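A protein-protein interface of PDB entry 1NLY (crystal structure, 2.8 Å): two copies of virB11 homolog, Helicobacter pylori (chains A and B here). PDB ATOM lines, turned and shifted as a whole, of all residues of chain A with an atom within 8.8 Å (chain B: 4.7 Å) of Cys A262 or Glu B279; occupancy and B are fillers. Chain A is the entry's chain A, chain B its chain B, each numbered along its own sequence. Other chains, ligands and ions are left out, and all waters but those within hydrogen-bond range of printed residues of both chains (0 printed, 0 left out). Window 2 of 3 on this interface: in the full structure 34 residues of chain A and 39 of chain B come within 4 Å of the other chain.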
ATOM      1  N   ASN A 173     -14.245  19.250 -21.310  1.00  0.00           N
ATOM      2  CA  ASN A 173     -12.814  19.399 -21.522  1.00  0.00           C
ATOM      3  C   ASN A 173     -12.518  18.333 -22.520  1.00  0.00           C
ATOM      4  O   ASN A 173     -12.788  17.156 -22.273  1.00  0.00           O
ATOM      5  CB  ASN A 173     -12.062  19.181 -20.216  1.00  0.00           C
ATOM      6  CG  ASN A 173     -12.247  20.344 -19.232  1.00  0.00           C
ATOM      7  OD1 ASN A 173     -11.659  21.399 -19.381  1.00  0.00           O
ATOM      8  ND2 ASN A 173     -13.058  20.128 -18.225  1.00  0.00           N
ATOM      9  N   TYR A 255       1.378  21.025 -15.811  1.00  0.00           N
ATOM     10  CA  TYR A 255       0.849  21.000 -14.460  1.00  0.00           C
ATOM     11  C   TYR A 255      -0.203  22.064 -14.194  1.00  0.00           C
ATOM     12  O   TYR A 255      -1.234  21.793 -13.579  1.00  0.00           O
ATOM     13  CB  TYR A 255       1.979  21.129 -13.437  1.00  0.00           C
ATOM     14  CG  TYR A 255       1.475  20.968 -12.021  1.00  0.00           C
ATOM     15  CD1 TYR A 255       0.895  19.778 -11.610  1.00  0.00           C
ATOM     16  CD2 TYR A 255       1.474  22.043 -11.128  1.00  0.00           C
ATOM     17  CE1 TYR A 255       0.315  19.660 -10.356  1.00  0.00           C
ATOM     18  CE2 TYR A 255       0.894  21.939  -9.866  1.00  0.00           C
ATOM     19  CZ  TYR A 255       0.314  20.748  -9.489  1.00  0.00           C
ATOM     20  OH  TYR A 255      -0.287  20.665  -8.255  1.00  0.00           O
ATOM     21  N   ASP A 256       0.054  23.278 -14.656  1.00  0.00           N
ATOM     22  CA  ASP A 256      -0.895  24.357 -14.448  1.00  0.00           C
ATOM     23  C   ASP A 256      -2.227  24.100 -15.111  1.00  0.00           C
ATOM     24  O   ASP A 256      -3.222  24.754 -14.812  1.00  0.00           O
ATOM     25  CB  ASP A 256      -0.317  25.653 -14.961  1.00  0.00           C
ATOM     26  CG  ASP A 256       0.948  25.990 -14.277  1.00  0.00           C
ATOM     27  OD1 ASP A 256       0.977  25.798 -13.040  1.00  0.00           O
ATOM     28  OD2 ASP A 256       1.890  26.440 -14.964  1.00  0.00           O
ATOM     29  N   PHE A 257      -2.227  23.147 -16.031  1.00  0.00           N
ATOM     30  CA  PHE A 257      -3.421  22.750 -16.751  1.00  0.00           C
ATOM     31  C   PHE A 257      -4.257  21.842 -15.828  1.00  0.00           C
ATOM     32  O   PHE A 257      -5.488  21.896 -15.826  1.00  0.00           O
ATOM     33  CB  PHE A 257      -2.986  22.045 -18.046  1.00  0.00           C
ATOM     34  CG  PHE A 257      -4.108  21.433 -18.813  1.00  0.00           C
ATOM     35  CD1 PHE A 257      -5.156  22.204 -19.276  1.00  0.00           C
ATOM     36  CD2 PHE A 257      -4.114  20.072 -19.081  1.00  0.00           C
ATOM     37  CE1 PHE A 257      -6.189  21.629 -19.984  1.00  0.00           C
ATOM     38  CE2 PHE A 257      -5.148  19.492 -19.787  1.00  0.00           C
ATOM     39  CZ  PHE A 257      -6.184  20.271 -20.242  1.00  0.00           C
ATOM     40  N   TYR A 258      -3.567  21.035 -15.025  1.00  0.00           N
ATOM     41  CA  TYR A 258      -4.192  20.115 -14.080  1.00  0.00           C
ATOM     42  C   TYR A 258      -4.961  20.892 -13.014  1.00  0.00           C
ATOM     43  O   TYR A 258      -6.105  20.581 -12.674  1.00  0.00           O
ATOM     44  CB  TYR A 258      -3.105  19.261 -13.423  1.00  0.00           C
ATOM     45  CG  TYR A 258      -3.593  18.347 -12.324  1.00  0.00           C
ATOM     46  CD1 TYR A 258      -4.564  17.373 -12.575  1.00  0.00           C
ATOM     47  CD2 TYR A 258      -3.063  18.436 -11.033  1.00  0.00           C
ATOM     48  CE1 TYR A 258      -4.988  16.504 -11.568  1.00  0.00           C
ATOM     49  CE2 TYR A 258      -3.477  17.583 -10.024  1.00  0.00           C
ATOM     50  CZ  TYR A 258      -4.439  16.615 -10.292  1.00  0.00           C
ATOM     51  OH  TYR A 258      -4.825  15.748  -9.286  1.00  0.00           O
ATOM     52  N   ASN A 259      -4.307  21.920 -12.499  1.00  0.00           N
ATOM     53  CA  ASN A 259      -4.899  22.746 -11.478  1.00  0.00           C
ATOM     54  C   ASN A 259      -6.097  23.463 -12.025  1.00  0.00           C
ATOM     55  O   ASN A 259      -7.087  23.617 -11.327  1.00  0.00           O
ATOM     56  CB  ASN A 259      -3.881  23.754 -10.949  1.00  0.00           C
ATOM     57  CG  ASN A 259      -2.694  23.080 -10.267  1.00  0.00           C
ATOM     58  OD1 ASN A 259      -2.833  21.986  -9.702  1.00  0.00           O
ATOM     59  ND2 ASN A 259      -1.520  23.734 -10.304  1.00  0.00           N
ATOM     60  N   VAL A 260      -6.005  23.890 -13.279  1.00  0.00           N
ATOM     61  CA  VAL A 260      -7.097  24.586 -13.928  1.00  0.00           C
ATOM     62  C   VAL A 260      -8.267  23.637 -14.056  1.00  0.00           C
ATOM     63  O   VAL A 260      -9.423  24.052 -13.988  1.00  0.00           O
ATOM     64  CB  VAL A 260      -6.684  25.097 -15.306  1.00  0.00           C
ATOM     65  CG1 VAL A 260      -7.863  25.713 -16.005  1.00  0.00           C
ATOM     66  CG2 VAL A 260      -5.613  26.132 -15.142  1.00  0.00           C
ATOM     67  N   LEU A 261      -7.967  22.356 -14.222  1.00  0.00           N
ATOM     68  CA  LEU A 261      -9.025  21.373 -14.336  1.00  0.00           C
ATOM     69  C   LEU A 261      -9.597  21.084 -12.959  1.00  0.00           C
ATOM     70  O   LEU A 261     -10.802  20.860 -12.823  1.00  0.00           O
ATOM     71  CB  LEU A 261      -8.492  20.097 -14.971  1.00  0.00           C
ATOM     72  CG  LEU A 261      -8.203  20.200 -16.468  1.00  0.00           C
ATOM     73  CD1 LEU A 261      -7.400  18.988 -16.920  1.00  0.00           C
ATOM     74  CD2 LEU A 261      -9.512  20.303 -17.231  1.00  0.00           C
ATOM     75  N   CYS A 262      -8.728  21.119 -11.946  1.00  0.00           N
ATOM     76  CA  CYS A 262      -9.118  20.878 -10.555  1.00  0.00           C
ATOM     77  C   CYS A 262     -10.009  21.953  -9.968  1.00  0.00           C
ATOM     78  O   CYS A 262     -10.721  21.689  -9.004  1.00  0.00           O
ATOM     79  CB  CYS A 262      -7.890  20.742  -9.668  1.00  0.00           C
ATOM     80  SG  CYS A 262      -7.028  19.220  -9.967  1.00  0.00           S
ATOM     81  N   SER A 263      -9.953  23.160 -10.529  1.00  0.00           N
ATOM     82  CA  SER A 263     -10.793  24.245 -10.050  1.00  0.00           C
ATOM     83  C   SER A 263     -12.135  24.146 -10.768  1.00  0.00           C
ATOM     84  O   SER A 263     -12.982  25.029 -10.637  1.00  0.00           O
ATOM     85  CB  SER A 263     -10.154  25.606 -10.332  1.00  0.00           C
ATOM     86  OG  SER A 263      -9.976  25.791 -11.712  1.00  0.00           O
ATOM     87  N   GLY A 264     -12.319  23.068 -11.524  1.00  0.00           N
ATOM     88  CA  GLY A 264     -13.558  22.870 -12.249  1.00  0.00           C
ATOM     89  C   GLY A 264     -13.777  23.919 -13.313  1.00  0.00           C
ATOM     90  O   GLY A 264     -14.831  24.510 -13.430  1.00  0.00           O
ATOM     91  N   HIS A 265     -12.777  24.130 -14.163  1.00  0.00           N
ATOM     92  CA  HIS A 265     -12.950  25.148 -15.188  1.00  0.00           C
ATOM     93  C   HIS A 265     -13.711  24.711 -16.429  1.00  0.00           C
ATOM     94  O   HIS A 265     -13.488  23.617 -16.953  1.00  0.00           O
ATOM     95  CB  HIS A 265     -11.601  25.776 -15.560  1.00  0.00           C
ATOM     96  CG  HIS A 265     -11.667  27.245 -15.806  1.00  0.00           C
ATOM     97  ND1 HIS A 265     -12.118  27.794 -16.996  1.00  0.00           N
ATOM     98  CD2 HIS A 265     -11.448  28.304 -14.990  1.00  0.00           C
ATOM     99  CE1 HIS A 265     -12.180  29.105 -16.894  1.00  0.00           C
ATOM    100  NE2 HIS A 265     -11.782  29.451 -15.677  1.00  0.00           N
ATOM    101  N   ILE A 297       3.577  15.404  -5.340  1.00  0.00           N
ATOM    102  CA  ILE A 297       2.367  14.706  -5.754  1.00  0.00           C
ATOM    103  C   ILE A 297       2.629  13.352  -6.430  1.00  0.00           C
ATOM    104  O   ILE A 297       3.328  13.268  -7.444  1.00  0.00           O
ATOM    105  CB  ILE A 297       1.511  15.612  -6.682  1.00  0.00           C
ATOM    106  CG1 ILE A 297       0.975  16.796  -5.870  1.00  0.00           C
ATOM    107  CG2 ILE A 297       0.364  14.816  -7.300  1.00  0.00           C
ATOM    108  CD1 ILE A 297      -0.031  17.649  -6.601  1.00  0.00           C
ATOM    109  N   SER A 301      -1.099   9.475  -8.984  1.00  0.00           N
ATOM    110  CA  SER A 301      -2.147  10.328  -8.436  1.00  0.00           C
ATOM    111  C   SER A 301      -2.557  11.355  -9.490  1.00  0.00           C
ATOM    112  O   SER A 301      -3.690  11.832  -9.493  1.00  0.00           O
ATOM    113  CB  SER A 301      -1.651  11.013  -7.165  1.00  0.00           C
ATOM    114  N   LEU A 302      -1.631  11.679 -10.391  1.00  0.00           N
ATOM    115  CA  LEU A 302      -1.905  12.623 -11.471  1.00  0.00           C
ATOM    116  C   LEU A 302      -2.754  11.944 -12.538  1.00  0.00           C
ATOM    117  O   LEU A 302      -3.784  12.477 -12.947  1.00  0.00           O
ATOM    118  CB  LEU A 302      -0.606  13.115 -12.102  1.00  0.00           C
ATOM    119  CG  LEU A 302       0.215  14.108 -11.290  1.00  0.00           C
ATOM    120  CD1 LEU A 302       1.581  14.308 -11.903  1.00  0.00           C
ATOM    121  CD2 LEU A 302      -0.527  15.410 -11.254  1.00  0.00           C
ATOM    122  N   GLU A 304      -4.775   9.464 -12.385  1.00  0.00           N
ATOM    123  CA  GLU A 304      -6.158   9.375 -11.951  1.00  0.00           C
ATOM    124  C   GLU A 304      -6.768  10.763 -11.985  1.00  0.00           C
ATOM    125  O   GLU A 304      -7.925  10.935 -12.362  1.00  0.00           O
ATOM    126  CB  GLU A 304      -6.265   8.789 -10.543  1.00  0.00           C
ATOM    127  CG  GLU A 304      -6.512   7.292 -10.553  1.00  0.00           C
ATOM    128  CD  GLU A 304      -7.019   6.745  -9.212  1.00  0.00           C
ATOM    129  OE1 GLU A 304      -8.046   7.236  -8.682  1.00  0.00           O
ATOM    130  OE2 GLU A 304      -6.393   5.800  -8.688  1.00  0.00           O
ATOM    131  N   GLY A 305      -5.970  11.757 -11.622  1.00  0.00           N
ATOM    132  CA  GLY A 305      -6.461  13.121 -11.619  1.00  0.00           C
ATOM    133  C   GLY A 305      -6.923  13.565 -12.990  1.00  0.00           C
ATOM    134  O   GLY A 305      -8.010  14.118 -13.142  1.00  0.00           O
ATOM    135  N   PHE A 306      -6.111  13.316 -14.006  1.00  0.00           N
ATOM    136  CA  PHE A 306      -6.491  13.726 -15.345  1.00  0.00           C
ATOM    137  C   PHE A 306      -7.661  12.913 -15.851  1.00  0.00           C
ATOM    138  O   PHE A 306      -8.459  13.384 -16.658  1.00  0.00           O
ATOM    139  CB  PHE A 306      -5.307  13.578 -16.305  1.00  0.00           C
ATOM    140  CG  PHE A 306      -4.338  14.746 -16.272  1.00  0.00           C
ATOM    141  CD1 PHE A 306      -3.150  14.676 -15.552  1.00  0.00           C
ATOM    142  CD2 PHE A 306      -4.628  15.920 -16.952  1.00  0.00           C
ATOM    143  CE1 PHE A 306      -2.268  15.767 -15.505  1.00  0.00           C
ATOM    144  CE2 PHE A 306      -3.764  17.008 -16.914  1.00  0.00           C
ATOM    145  CZ  PHE A 306      -2.576  16.934 -16.189  1.00  0.00           C
ATOM    146  N   ASP A 308     -10.214  12.000 -14.206  1.00  0.00           N
ATOM    147  CA  ASP A 308     -11.489  12.407 -13.622  1.00  0.00           C
ATOM    148  C   ASP A 308     -11.959  13.661 -14.336  1.00  0.00           C
ATOM    149  O   ASP A 308     -13.160  13.844 -14.584  1.00  0.00           O
ATOM    150  CB  ASP A 308     -11.343  12.726 -12.125  1.00  0.00           C
ATOM    151  CG  ASP A 308     -11.371  11.479 -11.244  1.00  0.00           C
ATOM    152  OD1 ASP A 308     -12.298  10.663 -11.422  1.00  0.00           O
ATOM    153  OD2 ASP A 308     -10.483  11.302 -10.374  1.00  0.00           O
ATOM    154  N   LEU A 309     -10.975  14.493 -14.690  1.00  0.00           N
ATOM    155  CA  LEU A 309     -11.182  15.791 -15.326  1.00  0.00           C
ATOM    156  C   LEU A 309     -11.437  15.827 -16.827  1.00  0.00           C
ATOM    157  O   LEU A 309     -12.339  16.539 -17.275  1.00  0.00           O
ATOM    158  CB  LEU A 309      -9.992  16.692 -14.988  1.00  0.00           C
ATOM    159  CG  LEU A 309      -9.679  16.633 -13.493  1.00  0.00           C
ATOM    160  CD1 LEU A 309      -8.375  17.315 -13.190  1.00  0.00           C
ATOM    161  CD2 LEU A 309     -10.805  17.272 -12.721  1.00  0.00           C
ATOM    162  N   ILE A 310     -10.664  15.072 -17.605  1.00  0.00           N
ATOM    163  CA  ILE A 310     -10.842  15.083 -19.056  1.00  0.00           C
ATOM    164  C   ILE A 310     -12.116  14.346 -19.481  1.00  0.00           C
ATOM    165  O   ILE A 310     -12.251  13.134 -19.312  1.00  0.00           O
ATOM    166  CB  ILE A 310      -9.607  14.492 -19.770  1.00  0.00           C
ATOM    167  CG1 ILE A 310      -8.336  15.203 -19.289  1.00  0.00           C
ATOM    168  CG2 ILE A 310      -9.751  14.649 -21.275  1.00  0.00           C
ATOM    169  CD1 ILE A 310      -8.311  16.699 -19.549  1.00  0.00           C
ATOM    170  N   HIS B 273     -11.464  28.388  -5.589  1.00  0.00           N
ATOM    171  CA  HIS B 273     -11.808  27.942  -6.929  1.00  0.00           C
ATOM    172  C   HIS B 273     -11.789  26.422  -6.914  1.00  0.00           C
ATOM    173  O   HIS B 273     -10.733  25.782  -6.854  1.00  0.00           O
ATOM    174  CB  HIS B 273     -10.790  28.416  -7.954  1.00  0.00           C
ATOM    175  CG  HIS B 273     -11.170  29.682  -8.654  1.00  0.00           C
ATOM    176  ND1 HIS B 273     -11.092  30.918  -8.050  1.00  0.00           N
ATOM    177  CD2 HIS B 273     -11.609  29.905  -9.915  1.00  0.00           C
ATOM    178  CE1 HIS B 273     -11.464  31.851  -8.911  1.00  0.00           C
ATOM    179  NE2 HIS B 273     -11.784  31.261 -10.049  1.00  0.00           N
ATOM    180  N   ALA B 274     -12.975  25.851  -6.945  1.00  0.00           N
ATOM    181  CA  ALA B 274     -13.120  24.413  -6.948  1.00  0.00           C
ATOM    182  C   ALA B 274     -14.497  24.155  -7.512  1.00  0.00           C
ATOM    183  O   ALA B 274     -15.423  24.939  -7.307  1.00  0.00           O
ATOM    184  CB  ALA B 274     -13.013  23.876  -5.546  1.00  0.00           C
ATOM    185  N   GLY B 275     -14.616  23.056  -8.241  1.00  0.00           N
ATOM    186  CA  GLY B 275     -15.875  22.708  -8.851  1.00  0.00           C
ATOM    187  C   GLY B 275     -16.779  21.914  -7.948  1.00  0.00           C
ATOM    188  O   GLY B 275     -17.916  21.640  -8.313  1.00  0.00           O
ATOM    189  N   SER B 276     -16.285  21.543  -6.771  1.00  0.00           N
ATOM    190  CA  SER B 276     -17.090  20.777  -5.820  1.00  0.00           C
ATOM    191  C   SER B 276     -16.390  20.462  -4.505  1.00  0.00           C
ATOM    192  O   SER B 276     -15.241  20.832  -4.272  1.00  0.00           O
ATOM    193  CB  SER B 276     -17.567  19.460  -6.446  1.00  0.00           C
ATOM    194  OG  SER B 276     -16.489  18.580  -6.723  1.00  0.00           O
ATOM    195  N   SER B 277     -17.116  19.772  -3.640  1.00  0.00           N
ATOM    196  CA  SER B 277     -16.597  19.395  -2.345  1.00  0.00           C
ATOM    197  C   SER B 277     -15.380  18.509  -2.528  1.00  0.00           C
ATOM    198  O   SER B 277     -14.275  18.873  -2.117  1.00  0.00           O
ATOM    199  CB  SER B 277     -17.667  18.642  -1.541  1.00  0.00           C
ATOM    200  OG  SER B 277     -17.073  17.645  -0.711  1.00  0.00           O
ATOM    201  N   GLU B 278     -15.578  17.351  -3.159  1.00  0.00           N
ATOM    202  CA  GLU B 278     -14.470  16.435  -3.347  1.00  0.00           C
ATOM    203  C   GLU B 278     -13.322  17.128  -4.051  1.00  0.00           C
ATOM    204  O   GLU B 278     -12.153  16.846  -3.762  1.00  0.00           O
ATOM    205  CB  GLU B 278     -14.871  15.196  -4.132  1.00  0.00           C
ATOM    206  CG  GLU B 278     -13.759  14.150  -4.100  1.00  0.00           C
ATOM    207  CD  GLU B 278     -13.225  13.888  -2.674  1.00  0.00           C
ATOM    208  OE1 GLU B 278     -13.945  13.256  -1.855  1.00  0.00           O
ATOM    209  OE2 GLU B 278     -12.081  14.327  -2.380  1.00  0.00           O
ATOM    210  N   GLU B 279     -13.645  18.034  -4.966  1.00  0.00           N
ATOM    211  CA  GLU B 279     -12.604  18.765  -5.668  1.00  0.00           C
ATOM    212  C   GLU B 279     -11.855  19.714  -4.719  1.00  0.00           C
ATOM    213  O   GLU B 279     -10.615  19.743  -4.688  1.00  0.00           O
ATOM    214  CB  GLU B 279     -13.211  19.548  -6.838  1.00  0.00           C
ATOM    215  CG  GLU B 279     -12.746  19.049  -8.215  1.00  0.00           C
ATOM    216  CD  GLU B 279     -13.548  19.601  -9.392  1.00  0.00           C
ATOM    217  OE1 GLU B 279     -13.692  20.839  -9.503  1.00  0.00           O
ATOM    218  OE2 GLU B 279     -14.016  18.780 -10.212  1.00  0.00           O
ATOM    219  N   ALA B 280     -12.599  20.484  -3.935  1.00  0.00           N
ATOM    220  CA  ALA B 280     -11.968  21.413  -3.011  1.00  0.00           C
ATOM    221  C   ALA B 280     -10.901  20.700  -2.168  1.00  0.00           C
ATOM    222  O   ALA B 280      -9.803  21.220  -1.939  1.00  0.00           O
ATOM    223  CB  ALA B 280     -13.015  22.020  -2.119  1.00  0.00           C
ATOM    224  N   PHE B 281     -11.233  19.497  -1.721  1.00  0.00           N
ATOM    225  CA  PHE B 281     -10.335  18.715  -0.893  1.00  0.00           C
ATOM    226  C   PHE B 281      -9.021  18.401  -1.592  1.00  0.00           C
ATOM    227  O   PHE B 281      -7.950  18.430  -0.970  1.00  0.00           O
ATOM    228  CB  PHE B 281     -11.048  17.429  -0.459  1.00  0.00           C
ATOM    229  CG  PHE B 281     -12.043  17.640   0.651  1.00  0.00           C
ATOM    230  CD1 PHE B 281     -13.299  17.030   0.614  1.00  0.00           C
ATOM    231  CD2 PHE B 281     -11.711  18.429   1.757  1.00  0.00           C
ATOM    232  CE1 PHE B 281     -14.219  17.211   1.662  1.00  0.00           C
ATOM    233  CE2 PHE B 281     -12.614  18.615   2.804  1.00  0.00           C
ATOM    234  CZ  PHE B 281     -13.868  18.001   2.758  1.00  0.00           C
ATOM    235  N   ILE B 282      -9.121  18.099  -2.885  1.00  0.00           N
ATOM    236  CA  ILE B 282      -7.966  17.763  -3.702  1.00  0.00           C
ATOM    237  C   ILE B 282      -7.232  19.057  -3.959  1.00  0.00           C
ATOM    238  O   ILE B 282      -6.016  19.123  -3.854  1.00  0.00           O
ATOM    239  CB  ILE B 282      -8.396  17.148  -5.044  1.00  0.00           C
ATOM    240  CG1 ILE B 282      -9.262  15.914  -4.774  1.00  0.00           C
ATOM    241  CG2 ILE B 282      -7.164  16.804  -5.872  1.00  0.00           C
ATOM    242  CD1 ILE B 282      -9.969  15.335  -5.992  1.00  0.00           C
ATOM    243  N   ARG B 283      -8.000  20.082  -4.290  1.00  0.00           N
ATOM    244  CA  ARG B 283      -7.492  21.416  -4.553  1.00  0.00           C
ATOM    245  C   ARG B 283      -6.562  21.880  -3.412  1.00  0.00           C
ATOM    246  O   ARG B 283      -5.493  22.459  -3.642  1.00  0.00           O
ATOM    247  CB  ARG B 283      -8.696  22.347  -4.655  1.00  0.00           C
ATOM    248  CG  ARG B 283      -8.536  23.556  -5.528  1.00  0.00           C
ATOM    249  CD  ARG B 283      -8.382  23.123  -6.944  1.00  0.00           C
ATOM    250  NE  ARG B 283      -6.990  23.198  -7.359  1.00  0.00           N
ATOM    251  CZ  ARG B 283      -6.280  24.322  -7.364  1.00  0.00           C
ATOM    252  NH1 ARG B 283      -6.839  25.468  -6.967  1.00  0.00           N
ATOM    253  NH2 ARG B 283      -5.023  24.300  -7.795  1.00  0.00           N
ATOM    254  N   ASN B 286      -3.222  19.798  -3.097  1.00  0.00           N
ATOM    255  CA  ASN B 286      -2.335  20.279  -4.145  1.00  0.00           C
ATOM    256  C   ASN B 286      -1.569  21.520  -3.709  1.00  0.00           C
ATOM    257  O   ASN B 286      -0.344  21.512  -3.646  1.00  0.00           O
ATOM    258  CB  ASN B 286      -3.146  20.632  -5.381  1.00  0.00           C
ATOM    259  CG  ASN B 286      -3.518  19.424  -6.192  1.00  0.00           C
ATOM    260  OD1 ASN B 286      -4.339  19.511  -7.109  1.00  0.00           O
ATOM    261  ND2 ASN B 286      -2.905  18.285  -5.876  1.00  0.00           N
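Among the printed residues, merely in contact across the chains: Ile A297 with Asn B286, Asn A259 with Arg B283, Cys A262 with Arg B283, Ser A263 with Gly B275, Ser A263 with His B273, Ser A263 with Ala B274, Tyr A258 with Asn B286, Ser A263 with Glu B279, Asn A259 with Asn B286, Ser A263 with Arg B283 and Cys A262 with Asn B286.
The backbone NH (N) of Gly A264 sits at hydrogen-bond distance from the side-chain carboxylate (OE1) of Glu B279 (3.3 Å). The side-chain carboxylate of Glu B279 sits close to the backbone carbonyl oxygen of Cys A262.
OH of Tyr A255 lies within hydrogen-bond range of OD1 of Asn A259 (3.2 Å). The side-chain sulfur of Cys A262 is in hydrogen-bond range of the backbone carbonyl oxygen of Tyr A258, at 3.2 Å. The backbone carbonyl oxygen (O) of Val A260 is in hydrogen-bond range of the side-chain hydroxyl (OG) of Ser A263 (2.9 Å). OE1 of Glu B279 lies within hydrogen-bond range of N of Gly B275, at 2.7 Å. The backbone NH (N) of Glu B279 lies within hydrogen-bond range of the side-chain hydroxyl (OG) of Ser B276, at 3.4 Å.
Along chain B the printed residues that touch a printed residue of chain A span positions 273 to 286. Hydrophobic or aromatic side chains of chain A within 4 Å of the printed part of chain B: Tyr A258 and Ile A297. Among the printed residues, no Asp or Glu carboxylate lies within 4 Å of a Lys or Arg side-chain nitrogen of the other chain.
Of chain B, only Glu B279, Arg B283 and Asn B286 come within 4 Å of Cys A262. Of chain A, only Cys A262, Ser A263 and Gly A264 come within 4 Å of Glu B279. No residue of chain A comes within 4 Å of Ser B276. No residue of chain A comes within 4 Å of Ala B280. No residue of chain A comes within 4 Å of Ile B282. Of the printed residues of chain B, Tyr A258 touches Asn B286 (3.6 Å). Printed residues of chain B within 4 Å of Ser A263: His B273 (3.5 Å), Ala B274 (3.6 Å), Gly B275 (3.5 Å), Glu B279 (3.9 Å) and Arg B283 (3.9 Å). Printed residues of chain B within 4 Å of Asn A259: Arg B283 and Asn B286. Of the printed residues of chain A, Gly B275 touches Ser A263. Glu A304 touches none of the printed residues of chain B. The nearest printed residue of chain B that does not touch Cys A262 is Ala B274 (4.2 Å).
No position is printed for both chains. Of the 13 pairs that touch across the chains among the printed residues, none has its exchanged pair printed and touching as well.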
